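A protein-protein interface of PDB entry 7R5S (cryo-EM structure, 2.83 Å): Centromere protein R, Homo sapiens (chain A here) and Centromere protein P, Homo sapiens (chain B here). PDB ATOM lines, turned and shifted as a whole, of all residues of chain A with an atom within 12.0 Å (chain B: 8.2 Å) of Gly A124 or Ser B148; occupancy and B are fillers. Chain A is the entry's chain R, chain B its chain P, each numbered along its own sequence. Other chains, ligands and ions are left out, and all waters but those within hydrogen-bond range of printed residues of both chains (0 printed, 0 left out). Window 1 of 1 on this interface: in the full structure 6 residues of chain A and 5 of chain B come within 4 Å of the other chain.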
ATOM      1  N   LEU A 113      25.398   8.378  10.903  1.00  0.00           N
ATOM      2  CA  LEU A 113      25.359   7.149  11.689  1.00  0.00           C
ATOM      3  C   LEU A 113      26.083   6.003  10.992  1.00  0.00           C
ATOM      4  O   LEU A 113      26.408   5.007  11.645  1.00  0.00           O
ATOM      5  CB  LEU A 113      23.911   6.762  12.011  1.00  0.00           C
ATOM      6  CG  LEU A 113      22.899   6.465  10.901  1.00  0.00           C
ATOM      7  CD1 LEU A 113      22.961   5.013  10.436  1.00  0.00           C
ATOM      8  CD2 LEU A 113      21.493   6.814  11.368  1.00  0.00           C
ATOM      9  N   SER A 116      29.694   3.720  12.003  1.00  0.00           N
ATOM     10  CA  SER A 116      29.656   3.352  13.418  1.00  0.00           C
ATOM     11  C   SER A 116      28.974   1.991  13.520  1.00  0.00           C
ATOM     12  O   SER A 116      27.750   1.882  13.447  1.00  0.00           O
ATOM     13  CB  SER A 116      28.927   4.410  14.234  1.00  0.00           C
ATOM     14  OG  SER A 116      27.532   4.171  14.230  1.00  0.00           O
ATOM     15  N   ARG A 117      29.782   0.942  13.686  1.00  0.00           N
ATOM     16  CA  ARG A 117      29.259  -0.413  13.816  1.00  0.00           C
ATOM     17  C   ARG A 117      28.410  -0.590  15.070  1.00  0.00           C
ATOM     18  O   ARG A 117      27.662  -1.567  15.164  1.00  0.00           O
ATOM     19  CB  ARG A 117      30.426  -1.408  13.814  1.00  0.00           C
ATOM     20  CG  ARG A 117      30.062  -2.893  13.897  1.00  0.00           C
ATOM     21  CD  ARG A 117      28.972  -3.293  12.908  1.00  0.00           C
ATOM     22  NE  ARG A 117      28.458  -4.634  13.173  1.00  0.00           N
ATOM     23  CZ  ARG A 117      28.030  -5.474  12.234  1.00  0.00           C
ATOM     24  NH1 ARG A 117      28.059  -5.117  10.959  1.00  0.00           N
ATOM     25  NH2 ARG A 117      27.577  -6.675  12.571  1.00  0.00           N
ATOM     26  N   GLU A 118      28.491   0.343  16.020  1.00  0.00           N
ATOM     27  CA  GLU A 118      27.774   0.210  17.283  1.00  0.00           C
ATOM     28  C   GLU A 118      26.260   0.180  17.103  1.00  0.00           C
ATOM     29  O   GLU A 118      25.555  -0.314  17.989  1.00  0.00           O
ATOM     30  CB  GLU A 118      28.189   1.344  18.223  1.00  0.00           C
ATOM     31  CG  GLU A 118      27.916   2.731  17.678  1.00  0.00           C
ATOM     32  CD  GLU A 118      27.907   3.785  18.765  1.00  0.00           C
ATOM     33  OE1 GLU A 118      27.491   4.928  18.487  1.00  0.00           O
ATOM     34  OE2 GLU A 118      28.332   3.469  19.895  1.00  0.00           O
ATOM     35  N   LEU A 119      25.742   0.695  15.987  1.00  0.00           N
ATOM     36  CA  LEU A 119      24.332   0.512  15.659  1.00  0.00           C
ATOM     37  C   LEU A 119      24.105  -0.601  14.645  1.00  0.00           C
ATOM     38  O   LEU A 119      23.028  -1.211  14.635  1.00  0.00           O
ATOM     39  CB  LEU A 119      23.718   1.810  15.123  1.00  0.00           C
ATOM     40  CG  LEU A 119      23.635   3.031  16.044  1.00  0.00           C
ATOM     41  CD1 LEU A 119      24.907   3.858  16.009  1.00  0.00           C
ATOM     42  CD2 LEU A 119      22.429   3.887  15.686  1.00  0.00           C
ATOM     43  N   GLU A 120      25.095  -0.881  13.792  1.00  0.00           N
ATOM     44  CA  GLU A 120      24.941  -1.900  12.762  1.00  0.00           C
ATOM     45  C   GLU A 120      24.970  -3.316  13.322  1.00  0.00           C
ATOM     46  O   GLU A 120      24.333  -4.206  12.747  1.00  0.00           O
ATOM     47  CB  GLU A 120      26.026  -1.735  11.696  1.00  0.00           C
ATOM     48  CG  GLU A 120      26.010  -0.374  11.017  1.00  0.00           C
ATOM     49  CD  GLU A 120      27.020  -0.267   9.894  1.00  0.00           C
ATOM     50  OE1 GLU A 120      27.731  -1.260   9.634  1.00  0.00           O
ATOM     51  OE2 GLU A 120      27.098   0.809   9.265  1.00  0.00           O
ATOM     52  N   ASN A 121      25.688  -3.553  14.423  1.00  0.00           N
ATOM     53  CA  ASN A 121      25.620  -4.851  15.083  1.00  0.00           C
ATOM     54  C   ASN A 121      24.329  -5.021  15.864  1.00  0.00           C
ATOM     55  O   ASN A 121      23.911  -6.156  16.115  1.00  0.00           O
ATOM     56  CB  ASN A 121      26.809  -5.040  16.028  1.00  0.00           C
ATOM     57  CG  ASN A 121      26.831  -4.019  17.151  1.00  0.00           C
ATOM     58  OD1 ASN A 121      26.228  -2.950  17.050  1.00  0.00           O
ATOM     59  ND2 ASN A 121      27.527  -4.347  18.232  1.00  0.00           N
ATOM     60  N   LEU A 122      23.694  -3.915  16.252  1.00  0.00           N
ATOM     61  CA  LEU A 122      22.441  -3.982  16.991  1.00  0.00           C
ATOM     62  C   LEU A 122      21.262  -4.206  16.054  1.00  0.00           C
ATOM     63  O   LEU A 122      20.381  -5.022  16.347  1.00  0.00           O
ATOM     64  CB  LEU A 122      22.252  -2.702  17.805  1.00  0.00           C
ATOM     65  CG  LEU A 122      22.946  -2.689  19.168  1.00  0.00           C
ATOM     66  CD1 LEU A 122      22.446  -1.533  20.019  1.00  0.00           C
ATOM     67  CD2 LEU A 122      22.760  -4.017  19.888  1.00  0.00           C
ATOM     68  N   ILE A 123      21.233  -3.500  14.920  1.00  0.00           N
ATOM     69  CA  ILE A 123      20.185  -3.740  13.937  1.00  0.00           C
ATOM     70  C   ILE A 123      20.374  -5.083  13.242  1.00  0.00           C
ATOM     71  O   ILE A 123      19.402  -5.661  12.747  1.00  0.00           O
ATOM     72  CB  ILE A 123      20.127  -2.593  12.911  1.00  0.00           C
ATOM     73  CG1 ILE A 123      21.403  -2.550  12.071  1.00  0.00           C
ATOM     74  CG2 ILE A 123      19.896  -1.261  13.613  1.00  0.00           C
ATOM     75  CD1 ILE A 123      21.219  -3.070  10.665  1.00  0.00           C
ATOM     76  N   GLY A 124      21.601  -5.595  13.194  1.00  0.00           N
ATOM     77  CA  GLY A 124      21.843  -6.948  12.739  1.00  0.00           C
ATOM     78  C   GLY A 124      22.830  -7.123  11.602  1.00  0.00           C
ATOM     79  O   GLY A 124      23.639  -8.053  11.643  1.00  0.00           O
ATOM     80  N   ILE A 125      22.792  -6.262  10.583  1.00  0.00           N
ATOM     81  CA  ILE A 125      23.767  -6.391   9.503  1.00  0.00           C
ATOM     82  C   ILE A 125      24.512  -5.081   9.266  1.00  0.00           C
ATOM     83  O   ILE A 125      25.720  -4.996   9.515  1.00  0.00           O
ATOM     84  CB  ILE A 125      23.090  -6.900   8.213  1.00  0.00           C
ATOM     85  CG1 ILE A 125      23.996  -6.677   6.997  1.00  0.00           C
ATOM     86  CG2 ILE A 125      21.707  -6.273   8.027  1.00  0.00           C
ATOM     87  CD1 ILE A 125      23.570  -7.452   5.771  1.00  0.00           C
ATOM     88  N   SER A 126      23.800  -4.050   8.811  1.00  0.00           N
ATOM     89  CA  SER A 126      24.381  -2.752   8.480  1.00  0.00           C
ATOM     90  C   SER A 126      23.255  -1.837   8.012  1.00  0.00           C
ATOM     91  O   SER A 126      22.138  -2.285   7.735  1.00  0.00           O
ATOM     92  CB  SER A 126      25.461  -2.849   7.398  1.00  0.00           C
ATOM     93  OG  SER A 126      25.038  -3.675   6.327  1.00  0.00           O
ATOM     94  N   CYS A 127      23.573  -0.547   7.907  1.00  0.00           N
ATOM     95  CA  CYS A 127      22.642   0.470   7.416  1.00  0.00           C
ATOM     96  C   CYS A 127      23.365   1.293   6.352  1.00  0.00           C
ATOM     97  O   CYS A 127      23.937   2.343   6.656  1.00  0.00           O
ATOM     98  CB  CYS A 127      22.135   1.346   8.558  1.00  0.00           C
ATOM     99  SG  CYS A 127      21.745   0.458  10.082  1.00  0.00           S
ATOM    100  N   ALA A 128      23.329   0.823   5.105  1.00  0.00           N
ATOM    101  CA  ALA A 128      24.010   1.516   4.012  1.00  0.00           C
ATOM    102  C   ALA A 128      23.429   1.026   2.693  1.00  0.00           C
ATOM    103  O   ALA A 128      23.519  -0.166   2.385  1.00  0.00           O
ATOM    104  CB  ALA A 128      25.515   1.277   4.073  1.00  0.00           C
ATOM    105  N   THR B 145      24.927 -14.912   2.895  1.00  0.00           N
ATOM    106  CA  THR B 145      23.656 -14.531   3.495  1.00  0.00           C
ATOM    107  C   THR B 145      23.790 -13.146   4.126  1.00  0.00           C
ATOM    108  O   THR B 145      24.789 -12.444   3.941  1.00  0.00           O
ATOM    109  CB  THR B 145      23.209 -15.580   4.510  1.00  0.00           C
ATOM    110  OG1 THR B 145      23.973 -15.438   5.714  1.00  0.00           O
ATOM    111  CG2 THR B 145      23.407 -16.980   3.952  1.00  0.00           C
ATOM    112  N   GLU B 146      22.777 -12.732   4.886  1.00  0.00           N
ATOM    113  CA  GLU B 146      22.778 -11.437   5.551  1.00  0.00           C
ATOM    114  C   GLU B 146      23.193 -11.526   7.014  1.00  0.00           C
ATOM    115  O   GLU B 146      23.137 -10.517   7.725  1.00  0.00           O
ATOM    116  CB  GLU B 146      21.398 -10.786   5.445  1.00  0.00           C
ATOM    117  N   CYS B 147      23.607 -12.700   7.480  1.00  0.00           N
ATOM    118  CA  CYS B 147      24.032 -12.875   8.863  1.00  0.00           C
ATOM    119  C   CYS B 147      25.489 -12.448   8.990  1.00  0.00           C
ATOM    120  O   CYS B 147      26.384 -13.105   8.446  1.00  0.00           O
ATOM    121  CB  CYS B 147      23.850 -14.324   9.309  1.00  0.00           C
ATOM    122  SG  CYS B 147      24.196 -14.612  11.061  1.00  0.00           S
ATOM    123  N   SER B 148      25.724 -11.349   9.709  1.00  0.00           N
ATOM    124  CA  SER B 148      27.077 -10.819   9.833  1.00  0.00           C
ATOM    125  C   SER B 148      27.866 -11.536  10.922  1.00  0.00           C
ATOM    126  O   SER B 148      29.084 -11.702  10.800  1.00  0.00           O
ATOM    127  CB  SER B 148      27.029  -9.317  10.112  1.00  0.00           C
ATOM    128  OG  SER B 148      28.236  -8.869  10.704  1.00  0.00           O
ATOM    129  N   GLU B 149      27.191 -11.965  11.991  1.00  0.00           N
ATOM    130  CA  GLU B 149      27.884 -12.678  13.058  1.00  0.00           C
ATOM    131  C   GLU B 149      28.380 -14.040  12.592  1.00  0.00           C
ATOM    132  O   GLU B 149      29.402 -14.531  13.087  1.00  0.00           O
ATOM    133  CB  GLU B 149      26.965 -12.826  14.272  1.00  0.00           C
ATOM    134  CG  GLU B 149      27.672 -13.287  15.534  1.00  0.00           C
ATOM    135  CD  GLU B 149      27.111 -12.636  16.782  1.00  0.00           C
ATOM    136  OE1 GLU B 149      27.880 -11.962  17.499  1.00  0.00           O
ATOM    137  OE2 GLU B 149      25.900 -12.792  17.042  1.00  0.00           O
ATOM    138  N   LEU B 150      27.685 -14.656  11.633  1.00  0.00           N
ATOM    139  CA  LEU B 150      28.154 -15.919  11.074  1.00  0.00           C
ATOM    140  C   LEU B 150      29.491 -15.734  10.366  1.00  0.00           C
ATOM    141  O   LEU B 150      30.435 -16.502  10.584  1.00  0.00           O
ATOM    142  CB  LEU B 150      27.103 -16.488  10.122  1.00  0.00           C
ATOM    143  CG  LEU B 150      27.293 -17.926   9.638  1.00  0.00           C
ATOM    144  CD1 LEU B 150      27.529 -18.861  10.812  1.00  0.00           C
ATOM    145  CD2 LEU B 150      26.077 -18.365   8.838  1.00  0.00           C
ATOM    146  N   SER B 151      29.596 -14.702   9.524  1.00  0.00           N
ATOM    147  CA  SER B 151      30.869 -14.411   8.869  1.00  0.00           C
ATOM    148  C   SER B 151      31.925 -13.964   9.872  1.00  0.00           C
ATOM    149  O   SER B 151      33.117 -14.237   9.680  1.00  0.00           O
ATOM    150  CB  SER B 151      30.674 -13.343   7.793  1.00  0.00           C
ATOM    151  OG  SER B 151      30.512 -12.061   8.373  1.00  0.00           O
ATOM    152  N   GLU B 152      31.512 -13.279  10.940  1.00  0.00           N
ATOM    153  CA  GLU B 152      32.455 -12.896  11.986  1.00  0.00           C
ATOM    154  C   GLU B 152      33.081 -14.127  12.629  1.00  0.00           C
ATOM    155  O   GLU B 152      34.306 -14.214  12.777  1.00  0.00           O
ATOM    156  CB  GLU B 152      31.749 -12.036  13.036  1.00  0.00           C
ATOM    157  CG  GLU B 152      32.654 -11.512  14.142  1.00  0.00           C
ATOM    158  CD  GLU B 152      34.018 -11.081  13.636  1.00  0.00           C
ATOM    159  OE1 GLU B 152      34.077 -10.277  12.681  1.00  0.00           O
ATOM    160  OE2 GLU B 152      35.032 -11.548  14.193  1.00  0.00           O
ATOM    161  N   PHE B 153      32.249 -15.100  13.010  1.00  0.00           N
ATOM    162  CA  PHE B 153      32.784 -16.339  13.564  1.00  0.00           C
ATOM    163  C   PHE B 153      33.584 -17.115  12.527  1.00  0.00           C
ATOM    164  O   PHE B 153      34.538 -17.814  12.881  1.00  0.00           O
ATOM    165  CB  PHE B 153      31.666 -17.220  14.121  1.00  0.00           C
ATOM    166  CG  PHE B 153      32.147 -18.567  14.575  1.00  0.00           C
ATOM    167  CD1 PHE B 153      32.747 -18.717  15.813  1.00  0.00           C
ATOM    168  CD2 PHE B 153      32.030 -19.677  13.754  1.00  0.00           C
ATOM    169  CE1 PHE B 153      33.205 -19.951  16.232  1.00  0.00           C
ATOM    170  CE2 PHE B 153      32.491 -20.910  14.164  1.00  0.00           C
ATOM    171  CZ  PHE B 153      33.078 -21.048  15.407  1.00  0.00           C
ATOM    172  N   VAL B 154      33.198 -17.028  11.252  1.00  0.00           N
ATOM    173  CA  VAL B 154      33.973 -17.677  10.198  1.00  0.00           C
ATOM    174  C   VAL B 154      35.393 -17.125  10.175  1.00  0.00           C
ATOM    175  O   VAL B 154      36.372 -17.879  10.154  1.00  0.00           O
ATOM    176  CB  VAL B 154      33.276 -17.507   8.836  1.00  0.00           C
ATOM    177  CG1 VAL B 154      34.276 -17.660   7.699  1.00  0.00           C
ATOM    178  CG2 VAL B 154      32.148 -18.515   8.691  1.00  0.00           C
ATOM    179  N   SER B 155      35.521 -15.798  10.200  1.00  0.00           N
ATOM    180  CA  SER B 155      36.844 -15.178  10.220  1.00  0.00           C
ATOM    181  C   SER B 155      37.594 -15.511  11.506  1.00  0.00           C
ATOM    182  O   SER B 155      38.818 -15.695  11.488  1.00  0.00           O
ATOM    183  CB  SER B 155      36.718 -13.665  10.047  1.00  0.00           C
ATOM    184  OG  SER B 155      36.421 -13.330   8.703  1.00  0.00           O
ATOM    185  N   ARG B 156      36.878 -15.596  12.629  1.00  0.00           N
ATOM    186  CA  ARG B 156      37.526 -15.932  13.895  1.00  0.00           C
ATOM    187  C   ARG B 156      38.107 -17.342  13.857  1.00  0.00           C
ATOM    188  O   ARG B 156      39.258 -17.562  14.248  1.00  0.00           O
ATOM    189  CB  ARG B 156      36.530 -15.788  15.046  1.00  0.00           C
ATOM    190  CG  ARG B 156      36.222 -14.348  15.423  1.00  0.00           C
ATOM    191  CD  ARG B 156      35.776 -14.240  16.869  1.00  0.00           C
ATOM    192  NE  ARG B 156      34.543 -14.981  17.119  1.00  0.00           N
ATOM    193  CZ  ARG B 156      33.346 -14.418  17.250  1.00  0.00           C
ATOM    194  NH1 ARG B 156      33.216 -13.102  17.156  1.00  0.00           N
ATOM    195  NH2 ARG B 156      32.278 -15.171  17.475  1.00  0.00           N
ATOM    196  N   PHE B 173      24.168 -23.132  16.498  1.00  0.00           N
ATOM    197  CA  PHE B 173      23.576 -21.969  15.848  1.00  0.00           C
ATOM    198  C   PHE B 173      22.389 -22.368  14.983  1.00  0.00           C
ATOM    199  O   PHE B 173      21.334 -21.727  15.030  1.00  0.00           O
ATOM    200  CB  PHE B 173      24.635 -21.245  15.016  1.00  0.00           C
ATOM    201  CG  PHE B 173      24.095 -20.102  14.205  1.00  0.00           C
ATOM    202  CD1 PHE B 173      23.867 -18.868  14.790  1.00  0.00           C
ATOM    203  CD2 PHE B 173      23.822 -20.258  12.857  1.00  0.00           C
ATOM    204  CE1 PHE B 173      23.373 -17.813  14.047  1.00  0.00           C
ATOM    205  CE2 PHE B 173      23.326 -19.208  12.109  1.00  0.00           C
ATOM    206  CZ  PHE B 173      23.102 -17.984  12.705  1.00  0.00           C
ATOM    207  N   CYS B 204      14.783 -11.832  12.559  1.00  0.00           N
ATOM    208  CA  CYS B 204      15.058 -11.597  13.972  1.00  0.00           C
ATOM    209  C   CYS B 204      13.984 -10.783  14.672  1.00  0.00           C
ATOM    210  O   CYS B 204      13.688 -11.040  15.840  1.00  0.00           O
ATOM    211  CB  CYS B 204      16.408 -10.887  14.133  1.00  0.00           C
ATOM    212  SG  CYS B 204      17.698 -11.475  13.012  1.00  0.00           S
ATOM    213  N   ARG B 223      17.515 -12.296  18.944  1.00  0.00           N
ATOM    214  CA  ARG B 223      18.806 -12.369  18.279  1.00  0.00           C
ATOM    215  C   ARG B 223      19.586 -13.575  18.783  1.00  0.00           C
ATOM    216  O   ARG B 223      19.322 -14.108  19.864  1.00  0.00           O
ATOM    217  CB  ARG B 223      19.623 -11.090  18.503  1.00  0.00           C
ATOM    218  CG  ARG B 223      19.072  -9.865  17.794  1.00  0.00           C
ATOM    219  CD  ARG B 223      19.398  -8.594  18.560  1.00  0.00           C
ATOM    220  NE  ARG B 223      20.818  -8.494  18.879  1.00  0.00           N
ATOM    221  CZ  ARG B 223      21.346  -7.540  19.639  1.00  0.00           C
ATOM    222  NH1 ARG B 223      20.569  -6.603  20.164  1.00  0.00           N
ATOM    223  NH2 ARG B 223      22.650  -7.525  19.879  1.00  0.00           N
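Of the 15 printed residues of chain B, 3 touch a printed residue of chain A. Hydrophobic or aromatic side chains of chain A within 4 Å of the printed part of chain B: Leu A122 and Ile A125.
Among the printed residues, merely in contact across the chains: Leu A122 with Arg B223, Ile A125 with Glu B146 and Gly A124 with Ser B148.
Of chain B, only Ser B148 comes within 4 Å of Gly A124. Printed residues of chain A within 4 Å of Ser B148: Arg A117 and Gly A124. Of chain A, only Ile A125 (3.7 Å) comes within 4 Å of Glu B146. No residue of chain A comes within 4 Å of Glu B149. No residue of chain A comes within 4 Å of Leu B150. No residue of chain A comes within 4 Å of Glu B152. Of the printed residues of chain B, Ile A125 touches Glu B146 (3.7 Å). Of the printed residues of chain B, Leu A122 touches Arg B223. Cys B204 touches none of the printed residues of chain A. The nearest residue of chain B that does not touch Gly A124 is Glu B146 (4.7 Å). The nearest residue of chain A that does not touch Ser B148 is Ile A125 (4.4 Å). The nearest printed residue of chain B that does not touch Arg A117 is Glu B149 (5.3 Å).
O of Ile A125 lies within hydrogen-bond range of NH1 of Arg A117. The side-chain amide oxygen of Asn A121 lies close to the backbone carbonyl oxygen of Arg A117 (2.7 Å). OG of Ser B151 lies within hydrogen-bond range of O of Ser B148, 2.8 Å away. The backbone carbonyl oxygen (O) of Glu A120 sits at hydrogen-bond distance from the backbone NH (N) of Ile A125.
The guanidinium group (NH2) of Arg A117 is in hydrogen-bond range of the side-chain hydroxyl (OG) of Ser B148.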
